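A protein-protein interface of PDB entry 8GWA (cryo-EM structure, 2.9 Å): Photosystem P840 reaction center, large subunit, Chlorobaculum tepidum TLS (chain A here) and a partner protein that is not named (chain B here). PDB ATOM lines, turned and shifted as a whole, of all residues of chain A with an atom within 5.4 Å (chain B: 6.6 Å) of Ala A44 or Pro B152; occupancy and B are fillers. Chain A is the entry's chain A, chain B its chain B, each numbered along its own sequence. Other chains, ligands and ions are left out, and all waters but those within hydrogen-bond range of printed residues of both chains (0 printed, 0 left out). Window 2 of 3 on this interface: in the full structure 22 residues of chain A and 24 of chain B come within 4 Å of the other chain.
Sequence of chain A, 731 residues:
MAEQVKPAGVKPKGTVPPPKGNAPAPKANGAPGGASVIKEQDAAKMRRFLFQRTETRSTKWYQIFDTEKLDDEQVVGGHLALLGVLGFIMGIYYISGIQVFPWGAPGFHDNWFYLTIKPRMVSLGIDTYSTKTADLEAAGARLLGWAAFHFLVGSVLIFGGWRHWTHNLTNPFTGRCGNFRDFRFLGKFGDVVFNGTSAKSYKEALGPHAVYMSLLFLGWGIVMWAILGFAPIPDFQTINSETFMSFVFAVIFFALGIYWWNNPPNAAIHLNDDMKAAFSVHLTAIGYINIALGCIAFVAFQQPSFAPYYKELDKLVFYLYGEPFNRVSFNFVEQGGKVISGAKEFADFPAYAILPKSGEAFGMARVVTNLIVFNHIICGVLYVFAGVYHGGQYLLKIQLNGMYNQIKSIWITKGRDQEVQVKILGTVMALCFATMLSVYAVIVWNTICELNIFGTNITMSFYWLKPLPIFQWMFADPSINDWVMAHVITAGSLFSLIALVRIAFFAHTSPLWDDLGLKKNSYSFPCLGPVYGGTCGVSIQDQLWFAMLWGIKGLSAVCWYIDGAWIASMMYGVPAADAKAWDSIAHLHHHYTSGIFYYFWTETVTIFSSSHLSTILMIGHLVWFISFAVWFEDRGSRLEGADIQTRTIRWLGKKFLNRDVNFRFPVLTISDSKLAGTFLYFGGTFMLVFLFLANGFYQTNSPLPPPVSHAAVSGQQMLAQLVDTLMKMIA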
ATOM      1  N   ASP A  42     -12.169  33.843  -8.716  1.00  0.00           N
ATOM      2  CA  ASP A  42     -13.238  34.248  -7.811  1.00  0.00           C
ATOM      3  C   ASP A  42     -12.893  33.855  -6.378  1.00  0.00           C
ATOM      4  O   ASP A  42     -13.770  33.767  -5.518  1.00  0.00           O
ATOM      5  CB  ASP A  42     -14.567  33.619  -8.237  1.00  0.00           C
ATOM      6  CG  ASP A  42     -15.766  34.314  -7.621  1.00  0.00           C
ATOM      7  OD1 ASP A  42     -15.637  35.495  -7.240  1.00  0.00           O
ATOM      8  OD2 ASP A  42     -16.835  33.676  -7.515  1.00  0.00           O
ATOM      9  N   ALA A  43     -11.604  33.603  -6.143  1.00  0.00           N
ATOM     10  CA  ALA A  43     -11.015  33.189  -4.872  1.00  0.00           C
ATOM     11  C   ALA A  43     -11.421  31.778  -4.471  1.00  0.00           C
ATOM     12  O   ALA A  43     -10.929  31.272  -3.455  1.00  0.00           O
ATOM     13  CB  ALA A  43     -11.349  34.150  -3.720  1.00  0.00           C
ATOM     14  N   ALA A  44     -12.294  31.124  -5.230  1.00  0.00           N
ATOM     15  CA  ALA A  44     -12.622  29.717  -5.045  1.00  0.00           C
ATOM     16  C   ALA A  44     -12.118  28.849  -6.182  1.00  0.00           C
ATOM     17  O   ALA A  44     -11.737  27.699  -5.954  1.00  0.00           O
ATOM     18  CB  ALA A  44     -14.137  29.535  -4.901  1.00  0.00           C
ATOM     19  N   LYS A  45     -12.105  29.383  -7.407  1.00  0.00           N
ATOM     20  CA  LYS A  45     -11.463  28.689  -8.516  1.00  0.00           C
ATOM     21  C   LYS A  45      -9.974  28.515  -8.253  1.00  0.00           C
ATOM     22  O   LYS A  45      -9.384  27.503  -8.653  1.00  0.00           O
ATOM     23  CB  LYS A  45     -11.720  29.451  -9.819  1.00  0.00           C
ATOM     24  CG  LYS A  45     -11.125  28.835 -11.082  1.00  0.00           C
ATOM     25  CD  LYS A  45      -9.755  29.410 -11.410  1.00  0.00           C
ATOM     26  CE  LYS A  45      -9.876  30.851 -11.881  1.00  0.00           C
ATOM     27  NZ  LYS A  45      -8.557  31.447 -12.224  1.00  0.00           N
ATOM     28  N   MET A  46      -9.353  29.487  -7.584  1.00  0.00           N
ATOM     29  CA  MET A  46      -7.995  29.293  -7.090  1.00  0.00           C
ATOM     30  C   MET A  46      -7.947  28.208  -6.023  1.00  0.00           C
ATOM     31  O   MET A  46      -6.985  27.435  -5.957  1.00  0.00           O
ATOM     32  CB  MET A  46      -7.443  30.603  -6.530  1.00  0.00           C
ATOM     33  CG  MET A  46      -6.049  30.471  -5.935  1.00  0.00           C
ATOM     34  SD  MET A  46      -5.684  31.739  -4.710  1.00  0.00           S
ATOM     35  CE  MET A  46      -6.195  33.204  -5.599  1.00  0.00           C
ATOM     36  N   ARG A  47      -8.974  28.138  -5.173  1.00  0.00           N
ATOM     37  CA  ARG A  47      -8.876  27.294  -3.988  1.00  0.00           C
ATOM     38  C   ARG A  47      -8.864  25.812  -4.352  1.00  0.00           C
ATOM     39  O   ARG A  47      -8.150  25.026  -3.720  1.00  0.00           O
ATOM     40  CB  ARG A  47     -10.001  27.627  -3.008  1.00  0.00           C
ATOM     41  CG  ARG A  47      -9.911  26.877  -1.690  1.00  0.00           C
ATOM     42  CD  ARG A  47     -11.028  27.278  -0.740  1.00  0.00           C
ATOM     43  NE  ARG A  47     -10.923  28.679  -0.351  1.00  0.00           N
ATOM     44  CZ  ARG A  47     -11.789  29.622  -0.695  1.00  0.00           C
ATOM     45  NH1 ARG A  47     -12.849  29.350  -1.437  1.00  0.00           N
ATOM     46  NH2 ARG A  47     -11.584  30.871  -0.284  1.00  0.00           N
ATOM     47  N   ARG A  48      -9.619  25.406  -5.372  1.00  0.00           N
ATOM     48  CA  ARG A  48      -9.439  24.044  -5.884  1.00  0.00           C
ATOM     49  C   ARG A  48      -8.387  24.004  -6.994  1.00  0.00           C
ATOM     50  O   ARG A  48      -8.511  23.348  -8.026  1.00  0.00           O
ATOM     51  CB  ARG A  48     -10.782  23.452  -6.322  1.00  0.00           C
ATOM     52  CG  ARG A  48     -11.319  23.747  -7.722  1.00  0.00           C
ATOM     53  CD  ARG A  48     -11.748  25.183  -7.891  1.00  0.00           C
ATOM     54  NE  ARG A  48     -12.420  25.388  -9.170  1.00  0.00           N
ATOM     55  CZ  ARG A  48     -11.795  25.553 -10.327  1.00  0.00           C
ATOM     56  NH1 ARG A  48     -10.475  25.542 -10.408  1.00  0.00           N
ATOM     57  NH2 ARG A  48     -12.513  25.732 -11.432  1.00  0.00           N
ATOM     58  N   PHE A  51      -5.923  23.155  -3.528  1.00  0.00           N
ATOM     59  CA  PHE A  51      -6.523  21.915  -3.039  1.00  0.00           C
ATOM     60  C   PHE A  51      -6.416  20.821  -4.095  1.00  0.00           C
ATOM     61  O   PHE A  51      -7.383  20.136  -4.427  1.00  0.00           O
ATOM     62  CB  PHE A  51      -7.976  22.147  -2.642  1.00  0.00           C
ATOM     63  CG  PHE A  51      -8.148  22.810  -1.306  1.00  0.00           C
ATOM     64  CD1 PHE A  51      -7.097  22.877  -0.408  1.00  0.00           C
ATOM     65  CD2 PHE A  51      -9.366  23.356  -0.943  1.00  0.00           C
ATOM     66  CE1 PHE A  51      -7.257  23.481   0.823  1.00  0.00           C
ATOM     67  CE2 PHE A  51      -9.532  23.962   0.286  1.00  0.00           C
ATOM     68  CZ  PHE A  51      -8.475  24.026   1.169  1.00  0.00           C
ATOM     69  N   ASP B 148      -8.372  20.987   4.099  1.00  0.00           N
ATOM     70  CA  ASP B 148      -7.910  20.565   2.780  1.00  0.00           C
ATOM     71  C   ASP B 148      -8.979  19.761   2.051  1.00  0.00           C
ATOM     72  O   ASP B 148      -9.066  19.803   0.818  1.00  0.00           O
ATOM     73  CB  ASP B 148      -6.623  19.753   2.908  1.00  0.00           C
ATOM     74  CG  ASP B 148      -5.444  20.595   3.353  1.00  0.00           C
ATOM     75  OD1 ASP B 148      -5.429  21.805   3.046  1.00  0.00           O
ATOM     76  OD2 ASP B 148      -4.531  20.045   4.002  1.00  0.00           O
ATOM     77  N   LYS B 149      -9.801  19.025   2.794  1.00  0.00           N
ATOM     78  CA  LYS B 149     -10.832  18.184   2.203  1.00  0.00           C
ATOM     79  C   LYS B 149     -12.179  18.881   2.072  1.00  0.00           C
ATOM     80  O   LYS B 149     -13.088  18.321   1.451  1.00  0.00           O
ATOM     81  CB  LYS B 149     -10.989  16.905   3.028  1.00  0.00           C
ATOM     82  CG  LYS B 149      -9.747  16.034   3.023  1.00  0.00           C
ATOM     83  CD  LYS B 149      -9.962  14.748   3.793  1.00  0.00           C
ATOM     84  CE  LYS B 149     -10.058  15.015   5.286  1.00  0.00           C
ATOM     85  NZ  LYS B 149      -8.776  15.517   5.851  1.00  0.00           N
ATOM     86  N   CYS B 150     -12.334  20.075   2.632  1.00  0.00           N
ATOM     87  CA  CYS B 150     -13.593  20.791   2.482  1.00  0.00           C
ATOM     88  C   CYS B 150     -13.687  21.401   1.083  1.00  0.00           C
ATOM     89  O   CYS B 150     -12.730  22.020   0.613  1.00  0.00           O
ATOM     90  CB  CYS B 150     -13.719  21.886   3.538  1.00  0.00           C
ATOM     91  SG  CYS B 150     -15.405  22.483   3.802  1.00  0.00           S
ATOM     92  N   PRO B 151     -14.813  21.223   0.396  1.00  0.00           N
ATOM     93  CA  PRO B 151     -14.954  21.759  -0.962  1.00  0.00           C
ATOM     94  C   PRO B 151     -14.756  23.262  -0.980  1.00  0.00           C
ATOM     95  O   PRO B 151     -15.273  23.978  -0.111  1.00  0.00           O
ATOM     96  CB  PRO B 151     -16.394  21.384  -1.342  1.00  0.00           C
ATOM     97  CG  PRO B 151     -16.712  20.213  -0.489  1.00  0.00           C
ATOM     98  CD  PRO B 151     -15.992  20.443   0.806  1.00  0.00           C
ATOM     99  N   PRO B 152     -14.003  23.778  -1.952  1.00  0.00           N
ATOM    100  CA  PRO B 152     -13.784  25.231  -2.018  1.00  0.00           C
ATOM    101  C   PRO B 152     -15.052  26.038  -2.217  1.00  0.00           C
ATOM    102  O   PRO B 152     -15.109  27.196  -1.784  1.00  0.00           O
ATOM    103  CB  PRO B 152     -12.828  25.375  -3.207  1.00  0.00           C
ATOM    104  CG  PRO B 152     -12.104  24.078  -3.234  1.00  0.00           C
ATOM    105  CD  PRO B 152     -13.143  23.055  -2.901  1.00  0.00           C
ATOM    106  N   LYS B 153     -16.072  25.471  -2.863  1.00  0.00           N
ATOM    107  CA  LYS B 153     -17.318  26.199  -3.057  1.00  0.00           C
ATOM    108  C   LYS B 153     -18.076  26.429  -1.757  1.00  0.00           C
ATOM    109  O   LYS B 153     -18.970  27.281  -1.728  1.00  0.00           O
ATOM    110  CB  LYS B 153     -18.209  25.458  -4.053  1.00  0.00           C
ATOM    111  CG  LYS B 153     -18.035  25.918  -5.491  1.00  0.00           C
ATOM    112  CD  LYS B 153     -18.673  27.281  -5.707  1.00  0.00           C
ATOM    113  CE  LYS B 153     -18.528  27.738  -7.148  1.00  0.00           C
ATOM    114  NZ  LYS B 153     -18.392  29.218  -7.245  1.00  0.00           N
ATOM    115  N   VAL B 154     -17.747  25.701  -0.693  1.00  0.00           N
ATOM    116  CA  VAL B 154     -18.345  25.899   0.623  1.00  0.00           C
ATOM    117  C   VAL B 154     -17.218  26.033   1.645  1.00  0.00           C
ATOM    118  O   VAL B 154     -16.573  25.044   2.012  1.00  0.00           O
ATOM    119  CB  VAL B 154     -19.335  24.779   0.994  1.00  0.00           C
ATOM    120  CG1 VAL B 154     -20.490  24.769   0.012  1.00  0.00           C
ATOM    121  CG2 VAL B 154     -18.681  23.403   0.949  1.00  0.00           C
ATOM    122  N   ASN B 155     -16.964  27.263   2.088  1.00  0.00           N
ATOM    123  CA  ASN B 155     -15.924  27.521   3.084  1.00  0.00           C
ATOM    124  C   ASN B 155     -16.448  27.215   4.488  1.00  0.00           C
ATOM    125  O   ASN B 155     -16.516  28.073   5.366  1.00  0.00           O
ATOM    126  CB  ASN B 155     -15.431  28.959   2.977  1.00  0.00           C
ATOM    127  CG  ASN B 155     -14.299  29.114   1.982  1.00  0.00           C
ATOM    128  OD1 ASN B 155     -14.400  29.879   1.023  1.00  0.00           O
ATOM    129  ND2 ASN B 155     -13.211  28.388   2.207  1.00  0.00           N
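Among the printed residues, 7 pairs touch across the chains. Among the printed residues, no Asp or Glu carboxylate lies within 4 Å of a Lys or Arg side-chain nitrogen of the other chain.
The backbone carbonyl oxygen (O) of Pro B152 lies within hydrogen-bond range of the guanidinium group (NH1) of Arg A47 (3.1 Å). The side-chain amide oxygen (OD1) of Asn B155 sits at hydrogen-bond distance from the guanidinium group (NH1) of Arg A47 (3.0 Å).
The side-chain sulfur (SG) of Cys B150 lies close to the backbone carbonyl oxygen (O) of Val B154 (3.3 Å). NH2 of Arg A47 is in hydrogen-bond range of O of Ala A43, at 3.3 Å. The backbone carbonyl oxygen (O) of Lys A45 is in hydrogen-bond range of the guanidinium group (NH1) of Arg A48, at 2.8 Å.
Ala A44 touches Pro B152. Arg A48 touches Pro B152 (CB to CG, 3.4 Å). Asp B148 touches Phe A51. Cys B150 touches Phe A51. Pro B152 touches Phe A51.
Of chain B, only Pro B152 comes within 4 Å of Ala A44. Of the printed residues of chain B, Arg A47 touches Pro B152 and Asn B155. Of the printed residues of chain B, Arg A48 touches Pro B152 (3.4 Å). Of chain A, only Ala A44, Arg A47, Arg A48 and Phe A51 come within 4 Å of Pro B152. The nearest printed residue of chain A that does not touch Pro B152 is Lys A45 (5.9 Å). The nearest printed residue of chain B that does not touch Phe A51 is Pro B151 (5.4 Å).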
